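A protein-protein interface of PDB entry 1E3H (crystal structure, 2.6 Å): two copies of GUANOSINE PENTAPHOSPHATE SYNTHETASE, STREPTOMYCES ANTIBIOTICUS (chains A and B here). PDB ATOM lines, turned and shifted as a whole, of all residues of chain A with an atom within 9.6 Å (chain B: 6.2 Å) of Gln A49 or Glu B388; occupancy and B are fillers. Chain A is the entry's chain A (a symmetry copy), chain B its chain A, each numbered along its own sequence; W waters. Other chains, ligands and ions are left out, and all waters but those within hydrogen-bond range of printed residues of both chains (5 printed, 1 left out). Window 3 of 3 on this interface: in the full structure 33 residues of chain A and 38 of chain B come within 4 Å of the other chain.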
ATOM      1  N   ASN A  20       9.243  16.836  -2.006  1.00  0.00           N
ATOM      2  CA  ASN A  20       9.987  15.704  -2.638  1.00  0.00           C
ATOM      3  C   ASN A  20       9.370  15.304  -3.987  1.00  0.00           C
ATOM      4  O   ASN A  20       8.690  14.279  -4.100  1.00  0.00           O
ATOM      5  CB  ASN A  20      10.000  14.494  -1.695  1.00  0.00           C
ATOM      6  CG  ASN A  20      10.925  13.384  -2.175  1.00  0.00           C
ATOM      7  OD1 ASN A  20      10.738  12.817  -3.258  1.00  0.00           O
ATOM      8  ND2 ASN A  20      11.931  13.066  -1.363  1.00  0.00           N
ATOM      9  N   GLY A  44      15.663  15.006  -8.084  1.00  0.00           N
ATOM     10  CA  GLY A  44      14.556  14.836  -7.167  1.00  0.00           C
ATOM     11  C   GLY A  44      14.297  13.431  -6.668  1.00  0.00           C
ATOM     12  O   GLY A  44      13.769  13.266  -5.567  1.00  0.00           O
ATOM     13  N   ARG A  45      14.643  12.407  -7.440  1.00  0.00           N
ATOM     14  CA  ARG A  45      14.385  11.068  -6.941  1.00  0.00           C
ATOM     15  C   ARG A  45      15.609  10.271  -6.491  1.00  0.00           C
ATOM     16  O   ARG A  45      15.497   9.431  -5.595  1.00  0.00           O
ATOM     17  CB  ARG A  45      13.570  10.256  -7.953  1.00  0.00           C
ATOM     18  CG  ARG A  45      14.238   9.991  -9.269  1.00  0.00           C
ATOM     19  CD  ARG A  45      13.569   8.810  -9.981  1.00  0.00           C
ATOM     20  NE  ARG A  45      14.453   8.274 -11.012  1.00  0.00           N
ATOM     21  CZ  ARG A  45      14.480   7.006 -11.406  1.00  0.00           C
ATOM     22  NH1 ARG A  45      13.666   6.110 -10.863  1.00  0.00           N
ATOM     23  NH2 ARG A  45      15.351   6.635 -12.337  1.00  0.00           N
ATOM     24  N   LEU A  46      16.773  10.547  -7.080  1.00  0.00           N
ATOM     25  CA  LEU A  46      18.007   9.836  -6.733  1.00  0.00           C
ATOM     26  C   LEU A  46      19.001  10.643  -5.901  1.00  0.00           C
ATOM     27  O   LEU A  46      19.171  11.841  -6.120  1.00  0.00           O
ATOM     28  CB  LEU A  46      18.705   9.367  -8.014  1.00  0.00           C
ATOM     29  CG  LEU A  46      18.482   7.939  -8.521  1.00  0.00           C
ATOM     30  CD1 LEU A  46      17.106   7.430  -8.165  1.00  0.00           C
ATOM     31  CD2 LEU A  46      18.690   7.923 -10.008  1.00  0.00           C
ATOM     32  N   ALA A  47      19.661   9.971  -4.955  1.00  0.00           N
ATOM     33  CA  ALA A  47      20.683  10.576  -4.092  1.00  0.00           C
ATOM     34  C   ALA A  47      20.282  11.914  -3.496  1.00  0.00           C
ATOM     35  O   ALA A  47      20.920  12.937  -3.736  1.00  0.00           O
ATOM     36  CB  ALA A  47      21.997  10.736  -4.869  1.00  0.00           C
ATOM     37  N   ARG A  48      19.241  11.890  -2.681  1.00  0.00           N
ATOM     38  CA  ARG A  48      18.737  13.099  -2.069  1.00  0.00           C
ATOM     39  C   ARG A  48      19.509  13.633  -0.866  1.00  0.00           C
ATOM     40  O   ARG A  48      19.169  14.693  -0.354  1.00  0.00           O
ATOM     41  CB  ARG A  48      17.270  12.881  -1.723  1.00  0.00           C
ATOM     42  CG  ARG A  48      16.486  12.525  -2.973  1.00  0.00           C
ATOM     43  CD  ARG A  48      15.015  12.274  -2.732  1.00  0.00           C
ATOM     44  NE  ARG A  48      14.781  11.066  -1.957  1.00  0.00           N
ATOM     45  CZ  ARG A  48      13.755  10.244  -2.160  1.00  0.00           C
ATOM     46  NH1 ARG A  48      12.873  10.501  -3.120  1.00  0.00           N
ATOM     47  NH2 ARG A  48      13.607   9.167  -1.392  1.00  0.00           N
ATOM     48  N   GLN A  49      20.550  12.932  -0.425  1.00  0.00           N
ATOM     49  CA  GLN A  49      21.316  13.412   0.726  1.00  0.00           C
ATOM     50  C   GLN A  49      22.499  14.267   0.299  1.00  0.00           C
ATOM     51  O   GLN A  49      23.086  14.970   1.114  1.00  0.00           O
ATOM     52  CB  GLN A  49      21.818  12.245   1.593  1.00  0.00           C
ATOM     53  CG  GLN A  49      20.738  11.247   1.986  1.00  0.00           C
ATOM     54  CD  GLN A  49      19.507  11.915   2.567  1.00  0.00           C
ATOM     55  OE1 GLN A  49      18.373  11.542   2.254  1.00  0.00           O
ATOM     56  NE2 GLN A  49      19.722  12.901   3.423  1.00  0.00           N
ATOM     57  N   ALA A  50      22.851  14.205  -0.980  1.00  0.00           N
ATOM     58  CA  ALA A  50      23.962  14.999  -1.497  1.00  0.00           C
ATOM     59  C   ALA A  50      23.532  16.459  -1.603  1.00  0.00           C
ATOM     60  O   ALA A  50      22.342  16.749  -1.769  1.00  0.00           O
ATOM     61  CB  ALA A  50      24.379  14.481  -2.871  1.00  0.00           C
ATOM     62  N   ALA A  51      24.492  17.376  -1.511  1.00  0.00           N
ATOM     63  CA  ALA A  51      24.185  18.798  -1.623  1.00  0.00           C
ATOM     64  C   ALA A  51      23.461  19.065  -2.941  1.00  0.00           C
ATOM     65  O   ALA A  51      22.549  19.890  -3.013  1.00  0.00           O
ATOM     66  CB  ALA A  51      25.463  19.619  -1.564  1.00  0.00           C
ATOM     67  N   GLY A  52      23.880  18.356  -3.982  1.00  0.00           N
ATOM     68  CA  GLY A  52      23.277  18.516  -5.288  1.00  0.00           C
ATOM     69  C   GLY A  52      23.370  17.207  -6.031  1.00  0.00           C
ATOM     70  O   GLY A  52      24.383  16.515  -5.962  1.00  0.00           O
ATOM     71  N   SER A  53      22.316  16.865  -6.756  1.00  0.00           N
ATOM     72  CA  SER A  53      22.281  15.616  -7.487  1.00  0.00           C
ATOM     73  C   SER A  53      21.494  15.783  -8.777  1.00  0.00           C
ATOM     74  O   SER A  53      20.474  16.469  -8.800  1.00  0.00           O
ATOM     75  CB  SER A  53      21.634  14.548  -6.607  1.00  0.00           C
ATOM     76  OG  SER A  53      21.314  13.391  -7.351  1.00  0.00           O
ATOM     77  N   ALA A  67      26.577  13.331  -8.363  1.00  0.00           N
ATOM     78  CA  ALA A  67      26.276  13.853  -7.042  1.00  0.00           C
ATOM     79  C   ALA A  67      27.414  14.758  -6.608  1.00  0.00           C
ATOM     80  O   ALA A  67      28.582  14.404  -6.728  1.00  0.00           O
ATOM     81  CB  ALA A  67      26.088  12.711  -6.045  1.00  0.00           C
ATOM     82  N   THR A  68      27.060  15.947  -6.134  1.00  0.00           N
ATOM     83  CA  THR A  68      28.041  16.905  -5.658  1.00  0.00           C
ATOM     84  C   THR A  68      27.846  17.133  -4.157  1.00  0.00           C
ATOM     85  O   THR A  68      26.738  17.387  -3.687  1.00  0.00           O
ATOM     86  CB  THR A  68      27.910  18.253  -6.395  1.00  0.00           C
ATOM     87  OG1 THR A  68      28.231  18.073  -7.779  1.00  0.00           O
ATOM     88  CG2 THR A  68      28.851  19.285  -5.794  1.00  0.00           C
ATOM     89  N   THR A  69      28.938  17.028  -3.412  1.00  0.00           N
ATOM     90  CA  THR A  69      28.899  17.241  -1.976  1.00  0.00           C
ATOM     91  C   THR A  69      29.972  18.263  -1.581  1.00  0.00           C
ATOM     92  O   THR A  69      30.940  18.486  -2.316  1.00  0.00           O
ATOM     93  CB  THR A  69      29.149  15.920  -1.225  1.00  0.00           C
ATOM     94  OG1 THR A  69      30.313  15.282  -1.764  1.00  0.00           O
ATOM     95  CG2 THR A  69      27.965  14.994  -1.372  1.00  0.00           C
ATOM     96  N   ALA A  70      29.786  18.890  -0.426  1.00  0.00           N
ATOM     97  CA  ALA A  70      30.735  19.881   0.072  1.00  0.00           C
ATOM     98  C   ALA A  70      30.943  19.676   1.563  1.00  0.00           C
ATOM     99  O   ALA A  70      30.008  19.315   2.281  1.00  0.00           O
ATOM    100  CB  ALA A  70      30.217  21.290  -0.196  1.00  0.00           C
ATOM    101  N   LYS A  72      31.362  20.364   5.486  1.00  0.00           N
ATOM    102  CA  LYS A  72      30.619  21.237   6.393  1.00  0.00           C
ATOM    103  C   LYS A  72      31.350  22.546   6.635  1.00  0.00           C
ATOM    104  O   LYS A  72      30.777  23.627   6.491  1.00  0.00           O
ATOM    105  CB  LYS A  72      30.398  20.536   7.740  1.00  0.00           C
ATOM    106  CG  LYS A  72      29.610  19.233   7.661  1.00  0.00           C
ATOM    107  CD  LYS A  72      28.185  19.455   7.149  1.00  0.00           C
ATOM    108  CE  LYS A  72      27.394  20.386   8.063  1.00  0.00           C
ATOM    109  NZ  LYS A  72      25.988  20.560   7.594  1.00  0.00           N
ATOM    110  N   ALA A 165      23.648  22.212  -6.107  1.00  0.00           N
ATOM    111  CA  ALA A 165      24.205  22.149  -4.756  1.00  0.00           C
ATOM    112  C   ALA A 165      24.244  23.509  -4.066  1.00  0.00           C
ATOM    113  O   ALA A 165      24.614  23.606  -2.898  1.00  0.00           O
ATOM    114  CB  ALA A 165      25.601  21.556  -4.800  1.00  0.00           C
ATOM    115  N   LYS A 269      16.356  24.780  -5.312  1.00  0.00           N
ATOM    116  CA  LYS A 269      17.094  24.414  -4.109  1.00  0.00           C
ATOM    117  C   LYS A 269      17.638  25.699  -3.479  1.00  0.00           C
ATOM    118  O   LYS A 269      17.762  26.724  -4.149  1.00  0.00           O
ATOM    119  CB  LYS A 269      18.246  23.456  -4.444  1.00  0.00           C
ATOM    120  CG  LYS A 269      17.802  22.075  -4.917  1.00  0.00           C
ATOM    121  CD  LYS A 269      18.965  21.078  -4.936  1.00  0.00           C
ATOM    122  CE  LYS A 269      18.524  19.708  -5.470  1.00  0.00           C
ATOM    123  NZ  LYS A 269      19.617  18.680  -5.495  1.00  0.00           N
ATOM    124  N   LYS B 305      13.361  16.801  11.634  1.00  0.00           N
ATOM    125  CA  LYS B 305      14.815  16.763  11.736  1.00  0.00           C
ATOM    126  C   LYS B 305      15.481  18.135  11.674  1.00  0.00           C
ATOM    127  O   LYS B 305      16.130  18.561  12.629  1.00  0.00           O
ATOM    128  CB  LYS B 305      15.403  15.858  10.648  1.00  0.00           C
ATOM    129  CG  LYS B 305      16.923  15.773  10.690  1.00  0.00           C
ATOM    130  CD  LYS B 305      17.463  14.690   9.770  1.00  0.00           C
ATOM    131  CE  LYS B 305      18.985  14.678   9.790  1.00  0.00           C
ATOM    132  NZ  LYS B 305      19.515  14.644  11.185  1.00  0.00           N
ATOM    133  N   ARG B 366       9.363   3.557   8.726  1.00  0.00           N
ATOM    134  CA  ARG B 366       9.414   4.799   7.962  1.00  0.00           C
ATOM    135  C   ARG B 366       8.722   4.614   6.615  1.00  0.00           C
ATOM    136  O   ARG B 366       8.367   3.498   6.243  1.00  0.00           O
ATOM    137  CB  ARG B 366      10.861   5.226   7.752  1.00  0.00           C
ATOM    138  CG  ARG B 366      11.488   5.774   9.006  1.00  0.00           C
ATOM    139  CD  ARG B 366      12.965   5.992   8.842  1.00  0.00           C
ATOM    140  NE  ARG B 366      13.676   4.727   8.722  1.00  0.00           N
ATOM    141  CZ  ARG B 366      14.978   4.633   8.481  1.00  0.00           C
ATOM    142  NH1 ARG B 366      15.702   5.735   8.334  1.00  0.00           N
ATOM    143  NH2 ARG B 366      15.557   3.442   8.386  1.00  0.00           N
ATOM    144  N   ARG B 386      13.147   3.481   2.224  1.00  0.00           N
ATOM    145  CA  ARG B 386      12.592   3.309   3.548  1.00  0.00           C
ATOM    146  C   ARG B 386      13.181   4.470   4.319  1.00  0.00           C
ATOM    147  O   ARG B 386      14.304   4.390   4.822  1.00  0.00           O
ATOM    148  CB  ARG B 386      13.051   1.981   4.142  1.00  0.00           C
ATOM    149  CG  ARG B 386      12.433   1.638   5.484  1.00  0.00           C
ATOM    150  CD  ARG B 386      13.002   0.333   5.974  1.00  0.00           C
ATOM    151  NE  ARG B 386      14.448   0.454   6.111  1.00  0.00           N
ATOM    152  CZ  ARG B 386      15.328  -0.434   5.663  1.00  0.00           C
ATOM    153  NH1 ARG B 386      14.918  -1.536   5.034  1.00  0.00           N
ATOM    154  NH2 ARG B 386      16.622  -0.211   5.852  1.00  0.00           N
ATOM    155  N   GLY B 387      12.426   5.561   4.395  1.00  0.00           N
ATOM    156  CA  GLY B 387      12.926   6.731   5.083  1.00  0.00           C
ATOM    157  C   GLY B 387      14.011   7.331   4.213  1.00  0.00           C
ATOM    158  O   GLY B 387      13.869   7.369   2.989  1.00  0.00           O
ATOM    159  N   GLU B 388      15.096   7.794   4.827  1.00  0.00           N
ATOM    160  CA  GLU B 388      16.196   8.380   4.068  1.00  0.00           C
ATOM    161  C   GLU B 388      17.075   7.314   3.403  1.00  0.00           C
ATOM    162  O   GLU B 388      17.925   7.632   2.566  1.00  0.00           O
ATOM    163  CB  GLU B 388      17.049   9.269   4.973  1.00  0.00           C
ATOM    164  CG  GLU B 388      16.381  10.591   5.321  1.00  0.00           C
ATOM    165  CD  GLU B 388      17.265  11.500   6.162  1.00  0.00           C
ATOM    166  OE1 GLU B 388      18.345  11.051   6.611  1.00  0.00           O
ATOM    167  OE2 GLU B 388      16.878  12.670   6.377  1.00  0.00           O
ATOM    168  N   THR B 389      16.870   6.055   3.780  1.00  0.00           N
ATOM    169  CA  THR B 389      17.634   4.956   3.209  1.00  0.00           C
ATOM    170  C   THR B 389      17.075   4.630   1.833  1.00  0.00           C
ATOM    171  O   THR B 389      15.896   4.298   1.687  1.00  0.00           O
ATOM    172  CB  THR B 389      17.580   3.695   4.112  1.00  0.00           C
ATOM    173  OG1 THR B 389      18.329   3.937   5.315  1.00  0.00           O
ATOM    174  CG2 THR B 389      18.160   2.477   3.385  1.00  0.00           C
ATOM    175  N   GLN B 390      17.930   4.747   0.824  1.00  0.00           N
ATOM    176  CA  GLN B 390      17.543   4.478  -0.550  1.00  0.00           C
ATOM    177  C   GLN B 390      18.584   3.577  -1.208  1.00  0.00           C
ATOM    178  O   GLN B 390      19.775   3.905  -1.255  1.00  0.00           O
ATOM    179  CB  GLN B 390      17.433   5.787  -1.327  1.00  0.00           C
ATOM    180  CG  GLN B 390      17.129   5.602  -2.801  1.00  0.00           C
ATOM    181  CD  GLN B 390      17.031   6.924  -3.544  1.00  0.00           C
ATOM    182  OE1 GLN B 390      18.018   7.650  -3.674  1.00  0.00           O
ATOM    183  NE2 GLN B 390      15.839   7.244  -4.033  1.00  0.00           N
ATOM    184  N   TYR B 426      28.598  10.546  -0.660  1.00  0.00           N
ATOM    185  CA  TYR B 426      27.423  11.387  -0.864  1.00  0.00           C
ATOM    186  C   TYR B 426      26.141  10.720  -0.373  1.00  0.00           C
ATOM    187  O   TYR B 426      25.081  11.352  -0.302  1.00  0.00           O
ATOM    188  CB  TYR B 426      27.297  11.803  -2.338  1.00  0.00           C
ATOM    189  CG  TYR B 426      27.037  10.693  -3.330  1.00  0.00           C
ATOM    190  CD1 TYR B 426      25.770  10.113  -3.448  1.00  0.00           C
ATOM    191  CD2 TYR B 426      28.055  10.245  -4.182  1.00  0.00           C
ATOM    192  CE1 TYR B 426      25.519   9.114  -4.396  1.00  0.00           C
ATOM    193  CE2 TYR B 426      27.819   9.249  -5.128  1.00  0.00           C
ATOM    194  CZ  TYR B 426      26.552   8.687  -5.231  1.00  0.00           C
ATOM    195  OH  TYR B 426      26.325   7.694  -6.159  1.00  0.00           O
ATOM    196  N   SER B 427      26.252   9.440  -0.031  1.00  0.00           N
ATOM    197  CA  SER B 427      25.129   8.666   0.487  1.00  0.00           C
ATOM    198  C   SER B 427      24.622   9.322   1.774  1.00  0.00           C
ATOM    199  O   SER B 427      23.447   9.200   2.134  1.00  0.00           O
ATOM    200  CB  SER B 427      25.588   7.239   0.787  1.00  0.00           C
ATOM    201  OG  SER B 427      24.570   6.493   1.420  1.00  0.00           O
ATOM    202  N   VAL B 428      25.525  10.011   2.468  1.00  0.00           N
ATOM    203  CA  VAL B 428      25.186  10.694   3.706  1.00  0.00           C
ATOM    204  C   VAL B 428      25.621  12.152   3.627  1.00  0.00           C
ATOM    205  O   VAL B 428      25.973  12.765   4.635  1.00  0.00           O
ATOM    206  CB  VAL B 428      25.866  10.036   4.926  1.00  0.00           C
ATOM    207  CG1 VAL B 428      25.373   8.611   5.089  1.00  0.00           C
ATOM    208  CG2 VAL B 428      27.382  10.072   4.765  1.00  0.00           C
ATOM    209  N   GLY B 429      25.618  12.691   2.412  1.00  0.00           N
ATOM    210  CA  GLY B 429      25.982  14.079   2.195  1.00  0.00           C
ATOM    211  C   GLY B 429      27.409  14.526   2.462  1.00  0.00           C
ATOM    212  O   GLY B 429      27.637  15.709   2.706  1.00  0.00           O
ATOM    213  N   GLU B 430      28.381  13.624   2.416  1.00  0.00           N
ATOM    214  CA  GLU B 430      29.743  14.068   2.661  1.00  0.00           C
ATOM    215  C   GLU B 430      30.768  13.654   1.612  1.00  0.00           C
ATOM    216  O   GLU B 430      30.470  12.879   0.708  1.00  0.00           O
ATOM    217  CB  GLU B 430      30.198  13.636   4.058  1.00  0.00           C
ATOM    218  CG  GLU B 430      29.961  12.194   4.402  1.00  0.00           C
ATOM    219  CD  GLU B 430      30.294  11.903   5.856  1.00  0.00           C
ATOM    220  OE1 GLU B 430      29.674  12.527   6.745  1.00  0.00           O
ATOM    221  OE2 GLU B 430      31.176  11.053   6.111  1.00  0.00           O
ATOM    222  N   LEU B 473      22.432   4.848  -2.396  1.00  0.00           N
ATOM    223  CA  LEU B 473      22.374   6.249  -2.809  1.00  0.00           C
ATOM    224  C   LEU B 473      21.963   7.199  -1.694  1.00  0.00           C
ATOM    225  O   LEU B 473      22.249   8.391  -1.747  1.00  0.00           O
ATOM    226  CB  LEU B 473      21.420   6.404  -3.988  1.00  0.00           C
ATOM    227  CG  LEU B 473      21.746   5.561  -5.217  1.00  0.00           C
ATOM    228  CD1 LEU B 473      20.722   5.870  -6.288  1.00  0.00           C
ATOM    229  CD2 LEU B 473      23.173   5.848  -5.713  1.00  0.00           C
ATOM    230  N   GLY B 474      21.275   6.659  -0.696  1.00  0.00           N
ATOM    231  CA  GLY B 474      20.845   7.439   0.447  1.00  0.00           C
ATOM    232  C   GLY B 474      20.987   6.532   1.648  1.00  0.00           C
ATOM    233  O   GLY B 474      20.630   5.356   1.573  1.00  0.00           O
ATOM    234  N   SER B 475      21.495   7.053   2.759  1.00  0.00           N
ATOM    235  CA  SER B 475      21.685   6.209   3.928  1.00  0.00           C
ATOM    236  C   SER B 475      21.329   6.824   5.277  1.00  0.00           C
ATOM    237  O   SER B 475      21.615   7.990   5.534  1.00  0.00           O
ATOM    238  CB  SER B 475      23.133   5.725   3.966  1.00  0.00           C
ATOM    239  OG  SER B 475      23.384   4.975   5.141  1.00  0.00           O
ATOM    240  N   ASN B 476      20.711   6.010   6.131  1.00  0.00           N
ATOM    241  CA  ASN B 476      20.312   6.402   7.484  1.00  0.00           C
ATOM    242  C   ASN B 476      19.434   5.320   8.115  1.00  0.00           C
ATOM    243  O   ASN B 476      18.292   5.574   8.483  1.00  0.00           O
ATOM    244  CB  ASN B 476      19.557   7.738   7.461  1.00  0.00           C
ATOM    245  CG  ASN B 476      19.048   8.152   8.841  1.00  0.00           C
ATOM    246  OD1 ASN B 476      19.756   8.031   9.847  1.00  0.00           O
ATOM    247  ND2 ASN B 476      17.815   8.658   8.888  1.00  0.00           N
HETATM  248  O   HOH W   1      27.095  17.935   0.871  1.00  0.00           O
HETATM  249  O   HOH W   2      21.432  10.995   5.044  1.00  0.00           O
HETATM  250  O   HOH W   3      14.917   8.317   0.697  1.00  0.00           O
HETATM  251  O   HOH W   4      17.499   9.477   0.839  1.00  0.00           O
HETATM  252  O   HOH W   5      18.903   9.292  -1.651  1.00  0.00           O
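Printed residues of chain B that touch a printed residue of chain A: Glu B388, Gln B390, Tyr B426, Ser B427, Gly B429, Glu B430 and Leu B473.
Hydrophobic or aromatic side chains of chain B that line the printed part of chain A: Tyr B426 and Leu B473.
Hydrophobic or aromatic side chains of chain A within 4 Å of the printed part of chain B: Leu A46, Ala A47, Ala A50 and Ala A67.
Among the printed residues, 16 pairs touch across the chains.
Among the printed residues, pairs that only touch across the chains: Gln A49 with Gly B429 (3.2 Å), Gln A49 with Ser B427 (3.4 Å), Thr A69 with Tyr B426 (3.4 Å), Ala A67 with Tyr B426 (3.5 Å), Ala A47 with Leu B473 (3.6 Å), Ala A50 with Tyr B426 (3.7 Å), Leu A46 with Gln B390 (3.8 Å), Gln A49 with Glu B388 (3.8 Å), Leu A46 with Leu B473 (3.8 Å), Gln A49 with Tyr B426 (3.9 Å), Thr A69 with Gly B429 (3.9 Å), Ala A47 with Tyr B426 (3.9 Å) and Arg A48 with Gln B390 (3.96 Å).
The side-chain carboxylate (OE1) of Glu B388 is in hydrogen-bond range of the side-chain amide nitrogen (ND2) of Asn B476 (3.3 Å).
The backbone carbonyl oxygen (O) of Gln B390 is in hydrogen-bond range of the backbone NH (N) of Leu B473, at 3.0 Å.
N of Gln B390 lies within hydrogen-bond range of O of Gly B474 (2.9 Å).
The backbone NH (N) of Ser B475 is in hydrogen-bond range of the backbone carbonyl oxygen (O) of Ser B427 (3.0 Å).
The side-chain amide oxygen (OD1) of Asn A20 sits at hydrogen-bond distance from the guanidinium group (NH1) of Arg A48 (3.2 Å).
O of Leu A46 lies within hydrogen-bond range of OG of Ser A53.
The side-chain amide nitrogen (NE2) of Gln B390 sits at hydrogen-bond distance from the backbone carbonyl oxygen (O) of Arg A45, at 2.7 Å.
OE1 of Gln B390 lies within hydrogen-bond range of N of Ala A47.
The side-chain hydroxyl (OG1) of Thr A69 lies within hydrogen-bond range of the backbone carbonyl oxygen (O) of Glu B430 (3.5 Å).
Water W4 bridges O of Glu B388 (2.6 Å) and OE1 of Gln A49 (2.7 Å).
Water W3 lies within hydrogen-bond range of the guanidinium group (NH2) of Arg A48 (2.6 Å) and the backbone carbonyl oxygen (O) of Gly B387 (2.7 Å).
Water W5 lies within hydrogen-bond range of the side-chain amide oxygen of Gln B390 (2.8 Å), the backbone NH of Arg A48 (2.8 Å), the backbone NH of Ala A47 (3.5 Å) and the backbone carbonyl oxygen of Leu B473 (3.5 Å).
Water W1 bridges the backbone carbonyl oxygen (O) of Gly B429 and the backbone NH (N) of Ala A70.
Water W2 lies within hydrogen-bond range of the side-chain amide nitrogen (NE2) of Gln A49, the backbone carbonyl oxygen (O) of Ser B475 and the side-chain carboxylate (OE1) of Glu B388.
Asn A20 touches none of the printed residues of chain B.
Of the printed residues of chain B, Arg A48 touches Gln B390 (3.96 Å).
Gly A52 touches none of the printed residues of chain B.
Printed residues of chain B within 4 Å of Thr A69: Tyr B426, Gly B429 and Glu B430.
Printed residues of chain A within 4 Å of Glu B388: Gln A49.
No residue of chain A comes within 4 Å of Thr B389.
Printed residues of chain A within 4 Å of Ser B427: Gln A49 (3.4 Å).
No residue of chain A comes within 4 Å of Gly B474.
The nearest residue of chain A that does not touch Glu B388 is Arg A48 (6.1 Å).
No position is printed for both chains.
Of the 16 pairs that touch across the chains among the printed residues, none has its exchanged pair printed and touching as well.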
